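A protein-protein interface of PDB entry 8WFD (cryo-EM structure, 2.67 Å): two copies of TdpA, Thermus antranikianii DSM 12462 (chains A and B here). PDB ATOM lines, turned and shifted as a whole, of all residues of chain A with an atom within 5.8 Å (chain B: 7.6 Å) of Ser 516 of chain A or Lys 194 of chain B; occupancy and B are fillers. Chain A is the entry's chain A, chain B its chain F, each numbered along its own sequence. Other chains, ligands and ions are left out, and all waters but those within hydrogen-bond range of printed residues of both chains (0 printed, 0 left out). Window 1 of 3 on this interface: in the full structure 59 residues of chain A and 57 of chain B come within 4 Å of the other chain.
No position is printed for both chains.
Of the 15 pairs that touch across the chains among the printed residues, none has its exchanged pair printed and touching as well.
Of chain B, only Lys 194 (3.6 Å) comes within 4 Å of Ser 516 of chain A.
Lys 194 of chain B touches five residues of chain A.
Printed residues of chain A within 4 Å of Glu 530 of chain B: Met 512.
Of the printed residues of chain A, Thr 195 of chain B touches Arg 188 (2.8 Å), Gln 517 (3.3 Å) and Glu 519 (3.9 Å).
Of the printed residues of chain A, Gln 505 of chain B touches Gln 517 (3.8 Å).
Of the printed residues of chain A, His 525 of chain B touches Glu 563.
Of the printed residues of chain A, Ser 527 of chain B touches Ala 538 and Lys 539.
Val 523 of chain B touches none of the printed residues of chain A.
Pro 511 of chain A touches none of the printed residues of chain B.
The nearest residue of chain A that does not touch Lys 194 of chain B is Glu 519 of chain A (4.6 Å).
NZ of Lys 194 of chain B sits at hydrogen-bond distance from OG of Ser 527 of chain B (3.4 Å).
The side-chain carboxylate (OE2) of Glu 519 of chain A is in salt-bridge range of the guanidinium group (NH2) of Arg 188 of chain A, at 3.1 Å.
OG of Ser 516 of chain A sits at hydrogen-bond distance from O of Met 512 of chain A.
A ring nitrogen (NE2) of His 525 of chain B sits at hydrogen-bond distance from the side-chain hydroxyl (OG) of Ser 527 of chain B, at 2.9 Å.
N of Lys 194 of chain B lies within hydrogen-bond range of O of His 525 of chain B (2.9 Å).
The side-chain amino group (NZ) of Lys 539 of chain A lies within salt-bridge range of the side-chain carboxylate (OE2) of Glu 563 of chain A (2.8 Å).
Hydrophobic or aromatic side chains of chain A that line the printed part of chain B: Met 512.
Hydrophobic or aromatic side chains of chain B that line the printed part of chain A: His 525 and Pro 553.
Among the printed residues, 15 pairs touch across the chains.
Among the printed residues, Asp or Glu carboxylates within 4 Å of a Lys or Arg side-chain nitrogen of the other chain: Glu 563 of chain A with Lys 194 of chain B (3.3 Å).
N of Thr 195 of chain B sits at hydrogen-bond distance from OE1 of Gln 517 of chain A (3.3 Å).
The side-chain carboxylate (OE1) of Glu 563 of chain A is in salt-bridge range of the side-chain amino group (NZ) of Lys 194 of chain B.
The side-chain amino group (NZ) of Lys 539 of chain A lies within hydrogen-bond range of the side-chain hydroxyl (OG) of Ser 527 of chain B, 2.9 Å away.
The backbone carbonyl oxygen (O) of Ala 538 of chain A lies close to the backbone carbonyl oxygen (O) of Ser 527 of chain B (3.5 Å).
The backbone carbonyl oxygen of Thr 518 of chain A is in hydrogen-bond range of the side-chain amino group of Lys 194 of chain B (3.0 Å).
Among the printed residues, pairs that only touch across the chains: Arg 188 of chain A with Thr 195 of chain B (2.8 Å), Met 512 of chain A with Ser 528 of chain B (3.6 Å), Ser 516 of chain A with Lys 194 of chain B (3.6 Å), Gln 517 of chain A with Lys 194 of chain B (3.6 Å), Glu 563 of chain A with Pro 553 of chain B (3.8 Å), Gln 517 of chain A with Gln 505 of chain B (3.8 Å), Glu 519 of chain A with Thr 195 of chain B (3.9 Å), Met 512 of chain A with Glu 530 of chain B (3.9 Å), Lys 539 of chain A with Lys 194 of chain B (3.97 Å) and Glu 563 of chain A with His 525 of chain B (3.998 Å).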
ATOM      1  N   ARG A 188     -20.049  -0.350  20.744  1.00  0.00           N
ATOM      2  CA  ARG A 188     -18.712  -0.793  21.115  1.00  0.00           C
ATOM      3  C   ARG A 188     -18.659  -1.113  22.602  1.00  0.00           C
ATOM      4  O   ARG A 188     -19.144  -0.338  23.435  1.00  0.00           O
ATOM      5  CB  ARG A 188     -17.674   0.267  20.757  1.00  0.00           C
ATOM      6  CG  ARG A 188     -17.316   0.260  19.295  1.00  0.00           C
ATOM      7  CD  ARG A 188     -18.391   1.016  18.580  1.00  0.00           C
ATOM      8  NE  ARG A 188     -18.399   2.410  18.986  1.00  0.00           N
ATOM      9  CZ  ARG A 188     -19.386   3.250  18.729  1.00  0.00           C
ATOM     10  NH1 ARG A 188     -20.502   2.847  18.144  1.00  0.00           N
ATOM     11  NH2 ARG A 188     -19.266   4.516  19.103  1.00  0.00           N
ATOM     12  N   PRO A 511      -6.101   3.746  21.687  1.00  0.00           N
ATOM     13  CA  PRO A 511      -6.120   5.183  21.394  1.00  0.00           C
ATOM     14  C   PRO A 511      -7.364   5.853  21.956  1.00  0.00           C
ATOM     15  O   PRO A 511      -8.446   5.266  22.011  1.00  0.00           O
ATOM     16  CB  PRO A 511      -6.101   5.236  19.862  1.00  0.00           C
ATOM     17  CG  PRO A 511      -5.630   3.889  19.427  1.00  0.00           C
ATOM     18  CD  PRO A 511      -6.110   2.931  20.462  1.00  0.00           C
ATOM     19  N   MET A 512      -7.196   7.107  22.378  1.00  0.00           N
ATOM     20  CA  MET A 512      -8.337   7.878  22.855  1.00  0.00           C
ATOM     21  C   MET A 512      -9.357   8.124  21.755  1.00  0.00           C
ATOM     22  O   MET A 512     -10.542   8.300  22.052  1.00  0.00           O
ATOM     23  CB  MET A 512      -7.861   9.205  23.446  1.00  0.00           C
ATOM     24  CG  MET A 512      -8.902   9.930  24.284  1.00  0.00           C
ATOM     25  SD  MET A 512      -9.665   8.895  25.545  1.00  0.00           S
ATOM     26  CE  MET A 512      -8.364   8.838  26.770  1.00  0.00           C
ATOM     27  N   GLU A 513      -8.929   8.122  20.491  1.00  0.00           N
ATOM     28  CA  GLU A 513      -9.869   8.271  19.388  1.00  0.00           C
ATOM     29  C   GLU A 513     -10.912   7.164  19.388  1.00  0.00           C
ATOM     30  O   GLU A 513     -12.064   7.399  19.007  1.00  0.00           O
ATOM     31  CB  GLU A 513      -9.116   8.286  18.059  1.00  0.00           C
ATOM     32  CG  GLU A 513      -8.167   9.460  17.905  1.00  0.00           C
ATOM     33  CD  GLU A 513      -6.791   9.180  18.475  1.00  0.00           C
ATOM     34  OE1 GLU A 513      -6.508   8.011  18.807  1.00  0.00           O
ATOM     35  OE2 GLU A 513      -5.991  10.130  18.595  1.00  0.00           O
ATOM     36  N   ILE A 514     -10.530   5.958  19.802  1.00  0.00           N
ATOM     37  CA  ILE A 514     -11.463   4.843  19.879  1.00  0.00           C
ATOM     38  C   ILE A 514     -12.054   4.680  21.275  1.00  0.00           C
ATOM     39  O   ILE A 514     -13.176   4.167  21.402  1.00  0.00           O
ATOM     40  CB  ILE A 514     -10.783   3.534  19.423  1.00  0.00           C
ATOM     41  CG1 ILE A 514     -10.633   3.528  17.902  1.00  0.00           C
ATOM     42  CG2 ILE A 514     -11.566   2.322  19.888  1.00  0.00           C
ATOM     43  CD1 ILE A 514      -9.948   2.306  17.360  1.00  0.00           C
ATOM     44  N   LEU A 515     -11.343   5.106  22.320  1.00  0.00           N
ATOM     45  CA  LEU A 515     -11.907   5.064  23.664  1.00  0.00           C
ATOM     46  C   LEU A 515     -13.055   6.051  23.825  1.00  0.00           C
ATOM     47  O   LEU A 515     -13.993   5.791  24.585  1.00  0.00           O
ATOM     48  CB  LEU A 515     -10.824   5.353  24.702  1.00  0.00           C
ATOM     49  CG  LEU A 515      -9.937   4.196  25.161  1.00  0.00           C
ATOM     50  CD1 LEU A 515      -8.939   4.678  26.196  1.00  0.00           C
ATOM     51  CD2 LEU A 515     -10.774   3.059  25.712  1.00  0.00           C
ATOM     52  N   SER A 516     -13.003   7.182  23.123  1.00  0.00           N
ATOM     53  CA  SER A 516     -14.021   8.211  23.272  1.00  0.00           C
ATOM     54  C   SER A 516     -15.303   7.897  22.516  1.00  0.00           C
ATOM     55  O   SER A 516     -16.283   8.635  22.662  1.00  0.00           O
ATOM     56  CB  SER A 516     -13.467   9.560  22.812  1.00  0.00           C
ATOM     57  OG  SER A 516     -13.153   9.539  21.434  1.00  0.00           O
ATOM     58  N   GLN A 517     -15.324   6.830  21.719  1.00  0.00           N
ATOM     59  CA  GLN A 517     -16.518   6.408  20.999  1.00  0.00           C
ATOM     60  C   GLN A 517     -17.123   5.131  21.566  1.00  0.00           C
ATOM     61  O   GLN A 517     -18.056   4.585  20.973  1.00  0.00           O
ATOM     62  CB  GLN A 517     -16.203   6.218  19.514  1.00  0.00           C
ATOM     63  CG  GLN A 517     -15.577   7.427  18.845  1.00  0.00           C
ATOM     64  CD  GLN A 517     -16.386   8.690  19.048  1.00  0.00           C
ATOM     65  OE1 GLN A 517     -17.613   8.651  19.103  1.00  0.00           O
ATOM     66  NE2 GLN A 517     -15.702   9.819  19.159  1.00  0.00           N
ATOM     67  N   THR A 518     -16.620   4.645  22.696  1.00  0.00           N
ATOM     68  CA  THR A 518     -17.111   3.415  23.299  1.00  0.00           C
ATOM     69  C   THR A 518     -18.282   3.712  24.225  1.00  0.00           C
ATOM     70  O   THR A 518     -18.254   4.677  24.992  1.00  0.00           O
ATOM     71  CB  THR A 518     -15.997   2.714  24.078  1.00  0.00           C
ATOM     72  OG1 THR A 518     -14.931   2.371  23.185  1.00  0.00           O
ATOM     73  CG2 THR A 518     -16.514   1.451  24.738  1.00  0.00           C
ATOM     74  N   GLU A 519     -19.316   2.877  24.146  1.00  0.00           N
ATOM     75  CA  GLU A 519     -20.491   3.026  24.993  1.00  0.00           C
ATOM     76  C   GLU A 519     -20.490   2.083  26.186  1.00  0.00           C
ATOM     77  O   GLU A 519     -20.810   2.509  27.298  1.00  0.00           O
ATOM     78  CB  GLU A 519     -21.771   2.805  24.184  1.00  0.00           C
ATOM     79  CG  GLU A 519     -22.010   3.826  23.093  1.00  0.00           C
ATOM     80  CD  GLU A 519     -21.689   3.283  21.721  1.00  0.00           C
ATOM     81  OE1 GLU A 519     -21.311   2.097  21.631  1.00  0.00           O
ATOM     82  OE2 GLU A 519     -21.819   4.031  20.731  1.00  0.00           O
ATOM     83  N   ALA A 538     -11.138   8.854  29.950  1.00  0.00           N
ATOM     84  CA  ALA A 538     -12.035   8.420  28.889  1.00  0.00           C
ATOM     85  C   ALA A 538     -13.503   8.424  29.293  1.00  0.00           C
ATOM     86  O   ALA A 538     -14.355   8.725  28.453  1.00  0.00           O
ATOM     87  CB  ALA A 538     -11.656   7.014  28.409  1.00  0.00           C
ATOM     88  N   LYS A 539     -13.820   8.094  30.544  1.00  0.00           N
ATOM     89  CA  LYS A 539     -15.212   8.039  30.991  1.00  0.00           C
ATOM     90  C   LYS A 539     -15.266   8.572  32.415  1.00  0.00           C
ATOM     91  O   LYS A 539     -14.665   7.987  33.319  1.00  0.00           O
ATOM     92  CB  LYS A 539     -15.754   6.614  30.905  1.00  0.00           C
ATOM     93  CG  LYS A 539     -17.199   6.455  31.336  1.00  0.00           C
ATOM     94  CD  LYS A 539     -18.081   7.530  30.736  1.00  0.00           C
ATOM     95  CE  LYS A 539     -18.322   7.287  29.262  1.00  0.00           C
ATOM     96  NZ  LYS A 539     -19.149   8.368  28.664  1.00  0.00           N
ATOM     97  N   GLU A 563     -24.211   2.931  28.152  1.00  0.00           N
ATOM     98  CA  GLU A 563     -24.860   4.169  27.754  1.00  0.00           C
ATOM     99  C   GLU A 563     -26.011   3.887  26.791  1.00  0.00           C
ATOM    100  O   GLU A 563     -25.943   2.952  25.992  1.00  0.00           O
ATOM    101  CB  GLU A 563     -23.866   5.101  27.078  1.00  0.00           C
ATOM    102  CG  GLU A 563     -23.179   6.082  27.996  1.00  0.00           C
ATOM    103  CD  GLU A 563     -22.356   7.089  27.226  1.00  0.00           C
ATOM    104  OE1 GLU A 563     -22.259   6.949  25.991  1.00  0.00           O
ATOM    105  OE2 GLU A 563     -21.804   8.016  27.852  1.00  0.00           O
ATOM    106  N   PHE B 192     -19.723  19.138  16.501  1.00  0.00           N
ATOM    107  CA  PHE B 192     -19.005  18.151  17.292  1.00  0.00           C
ATOM    108  C   PHE B 192     -19.974  17.375  18.172  1.00  0.00           C
ATOM    109  O   PHE B 192     -21.052  17.864  18.518  1.00  0.00           O
ATOM    110  CB  PHE B 192     -17.931  18.804  18.172  1.00  0.00           C
ATOM    111  CG  PHE B 192     -16.940  19.635  17.412  1.00  0.00           C
ATOM    112  CD1 PHE B 192     -16.152  19.069  16.427  1.00  0.00           C
ATOM    113  CD2 PHE B 192     -16.783  20.979  17.695  1.00  0.00           C
ATOM    114  CE1 PHE B 192     -15.238  19.830  15.737  1.00  0.00           C
ATOM    115  CE2 PHE B 192     -15.869  21.739  17.007  1.00  0.00           C
ATOM    116  CZ  PHE B 192     -15.096  21.165  16.028  1.00  0.00           C
ATOM    117  N   GLY B 193     -19.587  16.160  18.522  1.00  0.00           N
ATOM    118  CA  GLY B 193     -20.394  15.334  19.394  1.00  0.00           C
ATOM    119  C   GLY B 193     -20.082  13.871  19.214  1.00  0.00           C
ATOM    120  O   GLY B 193     -19.607  13.425  18.172  1.00  0.00           O
ATOM    121  N   LYS B 194     -20.364  13.106  20.264  1.00  0.00           N
ATOM    122  CA  LYS B 194     -20.148  11.673  20.217  1.00  0.00           C
ATOM    123  C   LYS B 194     -21.036  11.045  19.145  1.00  0.00           C
ATOM    124  O   LYS B 194     -21.958  11.666  18.617  1.00  0.00           O
ATOM    125  CB  LYS B 194     -20.428  11.055  21.585  1.00  0.00           C
ATOM    126  CG  LYS B 194     -19.797   9.702  21.791  1.00  0.00           C
ATOM    127  CD  LYS B 194     -19.780   9.331  23.254  1.00  0.00           C
ATOM    128  CE  LYS B 194     -19.695   7.829  23.432  1.00  0.00           C
ATOM    129  NZ  LYS B 194     -19.251   7.451  24.798  1.00  0.00           N
ATOM    130  N   THR B 195     -20.744   9.788  18.823  1.00  0.00           N
ATOM    131  CA  THR B 195     -21.480   9.090  17.778  1.00  0.00           C
ATOM    132  C   THR B 195     -22.856   8.686  18.292  1.00  0.00           C
ATOM    133  O   THR B 195     -22.969   7.968  19.291  1.00  0.00           O
ATOM    134  CB  THR B 195     -20.710   7.858  17.313  1.00  0.00           C
ATOM    135  OG1 THR B 195     -21.451   7.194  16.283  1.00  0.00           O
ATOM    136  CG2 THR B 195     -20.542   6.897  18.457  1.00  0.00           C
ATOM    137  N   GLY B 196     -23.899   9.139  17.603  1.00  0.00           N
ATOM    138  CA  GLY B 196     -25.264   8.813  17.948  1.00  0.00           C
ATOM    139  C   GLY B 196     -26.017   9.889  18.692  1.00  0.00           C
ATOM    140  O   GLY B 196     -27.083   9.599  19.245  1.00  0.00           O
ATOM    141  N   PHE B 197     -25.506  11.118  18.726  1.00  0.00           N
ATOM    142  CA  PHE B 197     -26.075  12.161  19.564  1.00  0.00           C
ATOM    143  C   PHE B 197     -26.711  13.301  18.779  1.00  0.00           C
ATOM    144  O   PHE B 197     -27.279  14.208  19.395  1.00  0.00           O
ATOM    145  CB  PHE B 197     -25.005  12.703  20.521  1.00  0.00           C
ATOM    146  CG  PHE B 197     -24.760  11.811  21.708  1.00  0.00           C
ATOM    147  CD1 PHE B 197     -23.982  10.677  21.586  1.00  0.00           C
ATOM    148  CD2 PHE B 197     -25.335  12.090  22.934  1.00  0.00           C
ATOM    149  CE1 PHE B 197     -23.769   9.847  22.665  1.00  0.00           C
ATOM    150  CE2 PHE B 197     -25.126  11.261  24.016  1.00  0.00           C
ATOM    151  CZ  PHE B 197     -24.343  10.141  23.882  1.00  0.00           C
ATOM    152  N   GLY B 198     -26.641  13.289  17.449  1.00  0.00           N
ATOM    153  CA  GLY B 198     -27.475  14.181  16.667  1.00  0.00           C
ATOM    154  C   GLY B 198     -26.810  15.121  15.680  1.00  0.00           C
ATOM    155  O   GLY B 198     -27.436  16.094  15.248  1.00  0.00           O
ATOM    156  N   LYS B 199     -25.563  14.851  15.295  1.00  0.00           N
ATOM    157  CA  LYS B 199     -24.878  15.732  14.353  1.00  0.00           C
ATOM    158  C   LYS B 199     -25.592  15.769  13.006  1.00  0.00           C
ATOM    159  O   LYS B 199     -25.859  16.847  12.460  1.00  0.00           O
ATOM    160  CB  LYS B 199     -23.430  15.283  14.169  1.00  0.00           C
ATOM    161  CG  LYS B 199     -22.577  15.366  15.416  1.00  0.00           C
ATOM    162  CD  LYS B 199     -21.119  15.108  15.090  1.00  0.00           C
ATOM    163  CE  LYS B 199     -20.881  13.677  14.652  1.00  0.00           C
ATOM    164  NZ  LYS B 199     -21.173  12.696  15.727  1.00  0.00           N
ATOM    165  N   GLN B 505     -16.931  14.632  14.994  1.00  0.00           N
ATOM    166  CA  GLN B 505     -17.031  13.786  16.183  1.00  0.00           C
ATOM    167  C   GLN B 505     -15.969  14.078  17.237  1.00  0.00           C
ATOM    168  O   GLN B 505     -16.063  13.576  18.360  1.00  0.00           O
ATOM    169  CB  GLN B 505     -16.915  12.301  15.823  1.00  0.00           C
ATOM    170  CG  GLN B 505     -18.196  11.581  15.468  1.00  0.00           C
ATOM    171  CD  GLN B 505     -17.962  10.096  15.267  1.00  0.00           C
ATOM    172  OE1 GLN B 505     -16.837   9.618  15.383  1.00  0.00           O
ATOM    173  NE2 GLN B 505     -19.022   9.360  14.962  1.00  0.00           N
ATOM    174  N   SER B 506     -14.965  14.883  16.910  1.00  0.00           N
ATOM    175  CA  SER B 506     -13.901  15.102  17.879  1.00  0.00           C
ATOM    176  C   SER B 506     -13.119  16.376  17.587  1.00  0.00           C
ATOM    177  O   SER B 506     -12.385  16.439  16.591  1.00  0.00           O
ATOM    178  CB  SER B 506     -12.954  13.902  17.902  1.00  0.00           C
ATOM    179  OG  SER B 506     -12.087  13.961  19.019  1.00  0.00           O
ATOM    180  N   VAL B 523     -22.021  22.014  19.703  1.00  0.00           N
ATOM    181  CA  VAL B 523     -21.326  20.944  20.412  1.00  0.00           C
ATOM    182  C   VAL B 523     -22.331  20.091  21.173  1.00  0.00           C
ATOM    183  O   VAL B 523     -23.091  20.606  21.996  1.00  0.00           O
ATOM    184  CB  VAL B 523     -20.260  21.509  21.366  1.00  0.00           C
ATOM    185  CG1 VAL B 523     -19.362  20.398  21.872  1.00  0.00           C
ATOM    186  CG2 VAL B 523     -19.444  22.583  20.670  1.00  0.00           C
ATOM    187  N   LYS B 524     -22.323  18.789  20.909  1.00  0.00           N
ATOM    188  CA  LYS B 524     -23.057  17.809  21.695  1.00  0.00           C
ATOM    189  C   LYS B 524     -22.106  17.128  22.677  1.00  0.00           C
ATOM    190  O   LYS B 524     -20.946  17.523  22.830  1.00  0.00           O
ATOM    191  CB  LYS B 524     -23.753  16.796  20.783  1.00  0.00           C
ATOM    192  CG  LYS B 524     -25.114  17.241  20.269  1.00  0.00           C
ATOM    193  CD  LYS B 524     -24.981  18.320  19.224  1.00  0.00           C
ATOM    194  CE  LYS B 524     -24.375  17.783  17.954  1.00  0.00           C
ATOM    195  NZ  LYS B 524     -24.285  18.847  16.929  1.00  0.00           N
ATOM    196  N   HIS B 525     -22.604  16.092  23.346  1.00  0.00           N
ATOM    197  CA  HIS B 525     -21.859  15.453  24.423  1.00  0.00           C
ATOM    198  C   HIS B 525     -20.507  14.942  23.941  1.00  0.00           C
ATOM    199  O   HIS B 525     -20.411  14.267  22.914  1.00  0.00           O
ATOM    200  CB  HIS B 525     -22.680  14.305  25.007  1.00  0.00           C
ATOM    201  CG  HIS B 525     -21.903  13.404  25.914  1.00  0.00           C
ATOM    202  ND1 HIS B 525     -21.445  13.807  27.150  1.00  0.00           N
ATOM    203  CD2 HIS B 525     -21.507  12.119  25.769  1.00  0.00           C
ATOM    204  CE1 HIS B 525     -20.796  12.810  27.724  1.00  0.00           C
ATOM    205  NE2 HIS B 525     -20.820  11.774  26.905  1.00  0.00           N
ATOM    206  N   LEU B 526     -19.459  15.265  24.698  1.00  0.00           N
ATOM    207  CA  LEU B 526     -18.122  14.727  24.494  1.00  0.00           C
ATOM    208  C   LEU B 526     -17.664  14.056  25.781  1.00  0.00           C
ATOM    209  O   LEU B 526     -17.701  14.671  26.851  1.00  0.00           O
ATOM    210  CB  LEU B 526     -17.131  15.821  24.087  1.00  0.00           C
ATOM    211  CG  LEU B 526     -17.491  16.705  22.892  1.00  0.00           C
ATOM    212  CD1 LEU B 526     -16.727  18.011  22.955  1.00  0.00           C
ATOM    213  CD2 LEU B 526     -17.217  15.988  21.586  1.00  0.00           C
ATOM    214  N   SER B 527     -17.230  12.799  25.676  1.00  0.00           N
ATOM    215  CA  SER B 527     -16.878  12.031  26.864  1.00  0.00           C
ATOM    216  C   SER B 527     -15.449  12.280  27.329  1.00  0.00           C
ATOM    217  O   SER B 527     -15.155  12.118  28.517  1.00  0.00           O
ATOM    218  CB  SER B 527     -17.077  10.538  26.603  1.00  0.00           C
ATOM    219  OG  SER B 527     -18.450  10.210  26.534  1.00  0.00           O
ATOM    220  N   SER B 528     -14.556  12.671  26.425  1.00  0.00           N
ATOM    221  CA  SER B 528     -13.134  12.745  26.727  1.00  0.00           C
ATOM    222  C   SER B 528     -12.755  14.113  27.278  1.00  0.00           C
ATOM    223  O   SER B 528     -13.280  15.142  26.845  1.00  0.00           O
ATOM    224  CB  SER B 528     -12.312  12.443  25.475  1.00  0.00           C
ATOM    225  OG  SER B 528     -10.927  12.482  25.756  1.00  0.00           O
ATOM    226  N   GLU B 529     -11.830  14.112  28.243  1.00  0.00           N
ATOM    227  CA  GLU B 529     -11.328  15.360  28.808  1.00  0.00           C
ATOM    228  C   GLU B 529     -10.501  16.144  27.799  1.00  0.00           C
ATOM    229  O   GLU B 529     -10.529  17.381  27.801  1.00  0.00           O
ATOM    230  CB  GLU B 529     -10.487  15.072  30.049  1.00  0.00           C
ATOM    231  CG  GLU B 529     -11.276  14.928  31.330  1.00  0.00           C
ATOM    232  CD  GLU B 529     -10.386  14.622  32.515  1.00  0.00           C
ATOM    233  OE1 GLU B 529      -9.195  14.996  32.474  1.00  0.00           O
ATOM    234  OE2 GLU B 529     -10.874  14.006  33.486  1.00  0.00           O
ATOM    235  N   GLU B 530      -9.750  15.447  26.947  1.00  0.00           N
ATOM    236  CA  GLU B 530      -8.927  16.123  25.955  1.00  0.00           C
ATOM    237  C   GLU B 530      -9.772  16.925  24.978  1.00  0.00           C
ATOM    238  O   GLU B 530      -9.376  18.025  24.575  1.00  0.00           O
ATOM    239  CB  GLU B 530      -8.073  15.102  25.204  1.00  0.00           C
ATOM    240  CG  GLU B 530      -6.936  14.519  26.027  1.00  0.00           C
ATOM    241  CD  GLU B 530      -7.268  13.154  26.608  1.00  0.00           C
ATOM    242  OE1 GLU B 530      -8.460  12.883  26.858  1.00  0.00           O
ATOM    243  OE2 GLU B 530      -6.332  12.354  26.819  1.00  0.00           O
ATOM    244  N   ASP B 531     -10.933  16.398  24.585  1.00  0.00           N
ATOM    245  CA  ASP B 531     -11.794  17.113  23.652  1.00  0.00           C
ATOM    246  C   ASP B 531     -12.270  18.434  24.237  1.00  0.00           C
ATOM    247  O   ASP B 531     -12.203  19.475  23.573  1.00  0.00           O
ATOM    248  CB  ASP B 531     -12.985  16.240  23.267  1.00  0.00           C
ATOM    249  CG  ASP B 531     -12.644  15.230  22.195  1.00  0.00           C
ATOM    250  OD1 ASP B 531     -11.587  15.379  21.550  1.00  0.00           O
ATOM    251  OD2 ASP B 531     -13.436  14.285  21.998  1.00  0.00           O
ATOM    252  N   PRO B 553     -24.613  12.861  29.285  1.00  0.00           N
ATOM    253  CA  PRO B 553     -24.863  12.250  27.960  1.00  0.00           C
ATOM    254  C   PRO B 553     -26.334  12.282  27.553  1.00  0.00           C
ATOM    255  O   PRO B 553     -27.098  11.332  27.721  1.00  0.00           O
ATOM    256  CB  PRO B 553     -24.357  10.819  28.151  1.00  0.00           C
ATOM    257  CG  PRO B 553     -24.494  10.557  29.597  1.00  0.00           C
ATOM    258  CD  PRO B 553     -24.268  11.855  30.303  1.00  0.00           C
